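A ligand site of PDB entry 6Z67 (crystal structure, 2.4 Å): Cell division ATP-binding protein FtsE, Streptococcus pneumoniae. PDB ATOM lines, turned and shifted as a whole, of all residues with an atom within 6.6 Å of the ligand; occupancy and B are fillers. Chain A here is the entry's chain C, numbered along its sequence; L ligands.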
ATOM      1  N   TYR A  13      12.211 -14.156 -27.785  1.00  0.00           N
ATOM      2  CA  TYR A  13      12.903 -13.673 -26.600  1.00  0.00           C
ATOM      3  C   TYR A  13      13.393 -12.250 -26.832  1.00  0.00           C
ATOM      4  O   TYR A  13      13.619 -11.825 -27.964  1.00  0.00           O
ATOM      5  CB  TYR A  13      14.066 -14.595 -26.237  1.00  0.00           C
ATOM      6  CG  TYR A  13      13.628 -15.953 -25.712  1.00  0.00           C
ATOM      7  CD1 TYR A  13      13.271 -16.113 -24.382  1.00  0.00           C
ATOM      8  CD2 TYR A  13      13.553 -17.049 -26.551  1.00  0.00           C
ATOM      9  CE1 TYR A  13      12.856 -17.341 -23.903  1.00  0.00           C
ATOM     10  CE2 TYR A  13      13.137 -18.284 -26.080  1.00  0.00           C
ATOM     11  CZ  TYR A  13      12.794 -18.425 -24.755  1.00  0.00           C
ATOM     12  OH  TYR A  13      12.380 -19.647 -24.268  1.00  0.00           O
ATOM     13  N   ASP A  14      13.544 -11.505 -25.730  1.00  0.00           N
ATOM     14  CA  ASP A  14      13.760 -10.063 -25.816  1.00  0.00           C
ATOM     15  C   ASP A  14      15.023  -9.698 -26.591  1.00  0.00           C
ATOM     16  O   ASP A  14      15.139  -8.553 -27.033  1.00  0.00           O
ATOM     17  CB  ASP A  14      13.801  -9.473 -24.414  1.00  0.00           C
ATOM     18  CG  ASP A  14      12.553  -9.802 -23.606  1.00  0.00           C
ATOM     19  OD1 ASP A  14      12.415 -10.956 -23.167  1.00  0.00           O
ATOM     20  OD2 ASP A  14      11.714  -8.895 -23.427  1.00  0.00           O
ATOM     21  N   ASN A  15      15.960 -10.626 -26.763  1.00  0.00           N
ATOM     22  CA  ASN A  15      17.159 -10.363 -27.537  1.00  0.00           C
ATOM     23  C   ASN A  15      16.937 -10.513 -29.041  1.00  0.00           C
ATOM     24  O   ASN A  15      17.907 -10.623 -29.790  1.00  0.00           O
ATOM     25  CB  ASN A  15      18.296 -11.279 -27.084  1.00  0.00           C
ATOM     26  CG  ASN A  15      17.985 -12.748 -27.294  1.00  0.00           C
ATOM     27  OD1 ASN A  15      16.903 -13.106 -27.753  1.00  0.00           O
ATOM     28  ND2 ASN A  15      18.946 -13.610 -26.946  1.00  0.00           N
ATOM     29  N   THR A  17      15.818 -13.054 -30.634  1.00  0.00           N
ATOM     30  CA  THR A  17      15.764 -14.451 -31.050  1.00  0.00           C
ATOM     31  C   THR A  17      14.330 -14.965 -30.998  1.00  0.00           C
ATOM     32  O   THR A  17      13.626 -14.774 -30.005  1.00  0.00           O
ATOM     33  CB  THR A  17      16.666 -15.303 -30.167  1.00  0.00           C
ATOM     34  OG1 THR A  17      17.842 -14.557 -29.809  1.00  0.00           O
ATOM     35  CG2 THR A  17      17.086 -16.574 -30.886  1.00  0.00           C
ATOM     36  N   THR A  18      13.909 -15.625 -32.076  1.00  0.00           N
ATOM     37  CA  THR A  18      12.569 -16.189 -32.189  1.00  0.00           C
ATOM     38  C   THR A  18      12.689 -17.709 -32.034  1.00  0.00           C
ATOM     39  O   THR A  18      13.080 -18.411 -32.968  1.00  0.00           O
ATOM     40  CB  THR A  18      11.924 -15.819 -33.521  1.00  0.00           C
ATOM     41  OG1 THR A  18      11.988 -14.402 -33.700  1.00  0.00           O
ATOM     42  CG2 THR A  18      10.470 -16.271 -33.559  1.00  0.00           C
ATOM     43  N   ALA A  19      12.361 -18.204 -30.845  1.00  0.00           N
ATOM     44  CA  ALA A  19      12.554 -19.622 -30.534  1.00  0.00           C
ATOM     45  C   ALA A  19      11.498 -20.492 -31.195  1.00  0.00           C
ATOM     46  O   ALA A  19      11.801 -21.600 -31.658  1.00  0.00           O
ATOM     47  CB  ALA A  19      12.551 -19.837 -29.025  1.00  0.00           C
ATOM     48  N   LEU A  20      10.252 -20.014 -31.253  1.00  0.00           N
ATOM     49  CA  LEU A  20       9.165 -20.707 -31.940  1.00  0.00           C
ATOM     50  C   LEU A  20       8.624 -19.787 -33.013  1.00  0.00           C
ATOM     51  O   LEU A  20       8.261 -18.643 -32.731  1.00  0.00           O
ATOM     52  CB  LEU A  20       8.052 -21.114 -30.975  1.00  0.00           C
ATOM     53  CG  LEU A  20       8.429 -22.056 -29.827  1.00  0.00           C
ATOM     54  CD1 LEU A  20       7.227 -22.287 -28.923  1.00  0.00           C
ATOM     55  CD2 LEU A  20       8.969 -23.370 -30.352  1.00  0.00           C
ATOM     56  N   GLY A  37      14.650 -33.183 -32.050  1.00  0.00           N
ATOM     57  CA  GLY A  37      15.158 -32.126 -32.880  1.00  0.00           C
ATOM     58  C   GLY A  37      16.555 -31.702 -32.458  1.00  0.00           C
ATOM     59  O   GLY A  37      17.002 -31.973 -31.345  1.00  0.00           O
ATOM     60  N   PRO A  38      17.272 -31.019 -33.350  1.00  0.00           N
ATOM     61  CA  PRO A  38      18.615 -30.540 -33.008  1.00  0.00           C
ATOM     62  C   PRO A  38      18.549 -29.519 -31.880  1.00  0.00           C
ATOM     63  O   PRO A  38      17.574 -28.774 -31.745  1.00  0.00           O
ATOM     64  CB  PRO A  38      19.116 -29.913 -34.315  1.00  0.00           C
ATOM     65  CG  PRO A  38      18.187 -30.405 -35.388  1.00  0.00           C
ATOM     66  CD  PRO A  38      16.873 -30.620 -34.721  1.00  0.00           C
ATOM     67  N   SER A  39      19.597 -29.503 -31.062  1.00  0.00           N
ATOM     68  CA  SER A  39      19.673 -28.545 -29.975  1.00  0.00           C
ATOM     69  C   SER A  39      19.496 -27.133 -30.505  1.00  0.00           C
ATOM     70  O   SER A  39      19.872 -26.820 -31.638  1.00  0.00           O
ATOM     71  CB  SER A  39      21.005 -28.671 -29.239  1.00  0.00           C
ATOM     72  OG  SER A  39      22.030 -27.952 -29.893  1.00  0.00           O
ATOM     73  N   GLY A  40      18.903 -26.276 -29.679  1.00  0.00           N
ATOM     74  CA  GLY A  40      18.569 -24.933 -30.108  1.00  0.00           C
ATOM     75  C   GLY A  40      17.345 -24.839 -30.999  1.00  0.00           C
ATOM     76  O   GLY A  40      16.933 -23.726 -31.343  1.00  0.00           O
ATOM     77  N   ALA A  41      16.752 -25.977 -31.392  1.00  0.00           N
ATOM     78  CA  ALA A  41      15.573 -25.946 -32.248  1.00  0.00           C
ATOM     79  C   ALA A  41      14.356 -25.388 -31.522  1.00  0.00           C
ATOM     80  O   ALA A  41      13.366 -25.038 -32.183  1.00  0.00           O
ATOM     81  CB  ALA A  41      15.269 -27.354 -32.759  1.00  0.00           C
ATOM     82  N   GLY A  42      14.394 -25.299 -30.196  1.00  0.00           N
ATOM     83  CA  GLY A  42      13.266 -24.829 -29.431  1.00  0.00           C
ATOM     84  C   GLY A  42      12.456 -25.917 -28.753  1.00  0.00           C
ATOM     85  O   GLY A  42      11.273 -25.678 -28.457  1.00  0.00           O
ATOM     86  N   LYS A  43      13.038 -27.087 -28.510  1.00  0.00           N
ATOM     87  CA  LYS A  43      12.305 -28.154 -27.844  1.00  0.00           C
ATOM     88  C   LYS A  43      11.838 -27.728 -26.458  1.00  0.00           C
ATOM     89  O   LYS A  43      10.667 -27.875 -26.101  1.00  0.00           O
ATOM     90  CB  LYS A  43      13.167 -29.416 -27.753  1.00  0.00           C
ATOM     91  CG  LYS A  43      13.490 -30.055 -29.088  1.00  0.00           C
ATOM     92  CD  LYS A  43      14.301 -31.328 -28.902  1.00  0.00           C
ATOM     93  CE  LYS A  43      15.641 -31.034 -28.259  1.00  0.00           C
ATOM     94  NZ  LYS A  43      16.404 -30.002 -29.017  1.00  0.00           N
ATOM     95  N   SER A  44      12.759 -27.183 -25.653  1.00  0.00           N
ATOM     96  CA  SER A  44      12.440 -26.832 -24.273  1.00  0.00           C
ATOM     97  C   SER A  44      11.583 -25.573 -24.179  1.00  0.00           C
ATOM     98  O   SER A  44      10.753 -25.471 -23.268  1.00  0.00           O
ATOM     99  CB  SER A  44      13.729 -26.665 -23.465  1.00  0.00           C
ATOM    100  OG  SER A  44      14.684 -27.631 -23.843  1.00  0.00           O
ATOM    101  N   THR A  45      11.768 -24.607 -25.081  1.00  0.00           N
ATOM    102  CA  THR A  45      10.806 -23.519 -25.172  1.00  0.00           C
ATOM    103  C   THR A  45       9.417 -24.049 -25.479  1.00  0.00           C
ATOM    104  O   THR A  45       8.417 -23.583 -24.909  1.00  0.00           O
ATOM    105  CB  THR A  45      11.239 -22.513 -26.241  1.00  0.00           C
ATOM    106  OG1 THR A  45      12.510 -21.946 -25.899  1.00  0.00           O
ATOM    107  CG2 THR A  45      10.203 -21.399 -26.372  1.00  0.00           C
ATOM    108  N   PHE A  46       9.336 -25.045 -26.363  1.00  0.00           N
ATOM    109  CA  PHE A  46       8.060 -25.671 -26.680  1.00  0.00           C
ATOM    110  C   PHE A  46       7.393 -26.236 -25.434  1.00  0.00           C
ATOM    111  O   PHE A  46       6.222 -25.954 -25.163  1.00  0.00           O
ATOM    112  CB  PHE A  46       8.269 -26.766 -27.735  1.00  0.00           C
ATOM    113  CG  PHE A  46       7.041 -27.580 -28.017  1.00  0.00           C
ATOM    114  CD1 PHE A  46       6.053 -27.105 -28.861  1.00  0.00           C
ATOM    115  CD2 PHE A  46       6.890 -28.837 -27.450  1.00  0.00           C
ATOM    116  CE1 PHE A  46       4.928 -27.863 -29.123  1.00  0.00           C
ATOM    117  CE2 PHE A  46       5.764 -29.601 -27.720  1.00  0.00           C
ATOM    118  CZ  PHE A  46       4.788 -29.116 -28.548  1.00  0.00           C
ATOM    119  N   ARG A  48       8.296 -25.811 -22.147  1.00  0.00           N
ATOM    120  CA  ARG A  48       8.152 -24.832 -21.080  1.00  0.00           C
ATOM    121  C   ARG A  48       6.899 -23.978 -21.270  1.00  0.00           C
ATOM    122  O   ARG A  48       6.277 -23.564 -20.291  1.00  0.00           O
ATOM    123  CB  ARG A  48       9.392 -23.947 -20.991  1.00  0.00           C
ATOM    124  CG  ARG A  48      10.630 -24.671 -20.502  1.00  0.00           C
ATOM    125  CD  ARG A  48      11.881 -23.812 -20.642  1.00  0.00           C
ATOM    126  NE  ARG A  48      11.930 -22.737 -19.664  1.00  0.00           N
ATOM    127  CZ  ARG A  48      12.157 -21.461 -19.965  1.00  0.00           C
ATOM    128  NH1 ARG A  48      12.349 -21.097 -21.226  1.00  0.00           N
ATOM    129  NH2 ARG A  48      12.183 -20.546 -19.007  1.00  0.00           N
ATOM    130  N   ASP A 164      11.191 -33.456 -19.539  1.00  0.00           N
ATOM    131  CA  ASP A 164      12.316 -32.917 -20.288  1.00  0.00           C
ATOM    132  C   ASP A 164      13.521 -33.842 -20.071  1.00  0.00           C
ATOM    133  O   ASP A 164      14.125 -33.840 -18.997  1.00  0.00           O
ATOM    134  CB  ASP A 164      12.632 -31.490 -19.860  1.00  0.00           C
ATOM    135  CG  ASP A 164      13.583 -30.788 -20.807  1.00  0.00           C
ATOM    136  OD1 ASP A 164      14.319 -31.480 -21.537  1.00  0.00           O
ATOM    137  OD2 ASP A 164      13.596 -29.540 -20.824  1.00  0.00           O
ATOM    138  N   ILE A 212      11.188 -30.827 -34.108  1.00  0.00           N
ATOM    139  CA  ILE A 212      11.297 -29.373 -34.245  1.00  0.00           C
ATOM    140  C   ILE A 212      12.661 -29.045 -34.829  1.00  0.00           C
ATOM    141  O   ILE A 212      13.680 -29.627 -34.422  1.00  0.00           O
ATOM    142  CB  ILE A 212      11.085 -28.650 -32.902  1.00  0.00           C
ATOM    143  CG1 ILE A 212       9.702 -28.980 -32.327  1.00  0.00           C
ATOM    144  CG2 ILE A 212      11.239 -27.150 -33.082  1.00  0.00           C
ATOM    145  CD1 ILE A 212       9.509 -28.507 -30.905  1.00  0.00           C
HETATM  146  P1  LIG L   1      16.469 -26.758 -27.299  1.00  0.00           P
HETATM  147  O1  LIG L   1      15.987 -27.393 -28.588  1.00  0.00           O
HETATM  148  O2  LIG L   1      17.946 -26.966 -27.074  1.00  0.00           O
HETATM  149  O3  LIG L   1      15.630 -27.149 -26.115  1.00  0.00           O
HETATM  150  P2  LIG L   1      15.848 -24.000 -26.474  1.00  0.00           P
HETATM  151  O4  LIG L   1      14.357 -23.936 -26.417  1.00  0.00           O
HETATM  152  O5  LIG L   1      16.589 -24.182 -25.192  1.00  0.00           O
HETATM  153  O6  LIG L   1      16.274 -25.167 -27.491  1.00  0.00           O
HETATM  154  O7  LIG L   1      16.403 -22.705 -27.234  1.00  0.00           O
HETATM  155  C1  LIG L   1      15.761 -22.287 -28.463  1.00  0.00           C
HETATM  156  C2  LIG L   1      16.347 -20.974 -28.914  1.00  0.00           C
HETATM  157  O8  LIG L   1      15.932 -19.931 -28.002  1.00  0.00           O
HETATM  158  C3  LIG L   1      17.887 -20.899 -28.935  1.00  0.00           C
HETATM  159  O9  LIG L   1      18.342 -20.066 -29.991  1.00  0.00           O
HETATM  160  C4  LIG L   1      18.206 -20.316 -27.558  1.00  0.00           C
HETATM  161  O10 LIG L   1      19.452 -19.652 -27.533  1.00  0.00           O
HETATM  162  C5  LIG L   1      17.045 -19.332 -27.382  1.00  0.00           C
HETATM  163  N1  LIG L   1      16.719 -19.053 -25.993  1.00  0.00           N
HETATM  164  C6  LIG L   1      16.348 -19.961 -25.040  1.00  0.00           C
HETATM  165  N2  LIG L   1      16.109 -19.421 -23.868  1.00  0.00           N
HETATM  166  C7  LIG L   1      16.344 -18.069 -24.064  1.00  0.00           C
HETATM  167  C8  LIG L   1      16.256 -16.962 -23.203  1.00  0.00           C
HETATM  168  N3  LIG L   1      15.917 -17.056 -21.917  1.00  0.00           N
HETATM  169  N4  LIG L   1      16.557 -15.749 -23.708  1.00  0.00           N
HETATM  170  C9  LIG L   1      16.904 -15.664 -25.001  1.00  0.00           C
HETATM  171  N5  LIG L   1      17.018 -16.628 -25.907  1.00  0.00           N
HETATM  172  C10 LIG L   1      16.718 -17.828 -25.372  1.00  0.00           C
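N of Thr 45 lies within hydrogen-bond range of O4 of the ligand, 3.0 Å away.
The backbone NH (N) of Ser 44 lies within hydrogen-bond range of an oxygen (O3) of the ligand (2.9 Å).
OG of Ser 44 lies within hydrogen-bond range of O3 of the ligand (2.5 Å).
An oxygen (O4) of the ligand lies within hydrogen-bond range of the side-chain hydroxyl of Thr 45 (2.8 Å).
An oxygen (O1) of the ligand lies within hydrogen-bond range of the backbone NH (N) of Gly 42, 3.1 Å away.
O1 of the ligand is in salt-bridge range of NZ of Lys 43 (2.7 Å).
The backbone NH (N) of Gly 40 sits at hydrogen-bond distance from an oxygen (O2) of the ligand (2.9 Å).
N of Lys 43 sits at hydrogen-bond distance from O1 of the ligand, 3.0 Å away.
The backbone NH (N) of Ala 41 is in hydrogen-bond range of an oxygen (O1) of the ligand, 3.2 Å away.
The side-chain amino group (NZ) of Lys 43 sits at hydrogen-bond distance from the backbone carbonyl oxygen (O) of Pro 38, 3.2 Å away.
The side-chain amide oxygen (OD1) of Asn 15 lies within hydrogen-bond range of the side-chain hydroxyl (OG1) of Thr 17.
The side-chain hydroxyl (OH) of Tyr 13 sits at hydrogen-bond distance from the side-chain hydroxyl (OG1) of Thr 45 (2.8 Å).
The side-chain amino group (NZ) of Lys 43 lies within hydrogen-bond range of the backbone carbonyl oxygen (O) of Gly 37 (3.1 Å).
NH1 of Arg 48 lies within hydrogen-bond range of OH of Tyr 13, 3.4 Å away.
Tyr 13 touches the ligand (CB to C9, 3.3 Å).
ND2 of Asn 15 touches C9 of the ligand, 3.5 Å away.
Thr 17 touches the ligand (CG2 to O9, 3.8 Å).
CB of Ala 19 touches O8 of the ligand (3.5 Å).
Pro 38 touches the ligand (O to O1, 3.8 Å).
Ser 39 touches the ligand.
Hydrophobic or aromatic side chains that line the ligand: Tyr 13 and Ala 19.
The nearest printed residue that does not touch the ligand is Arg 48 (4.9 Å).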
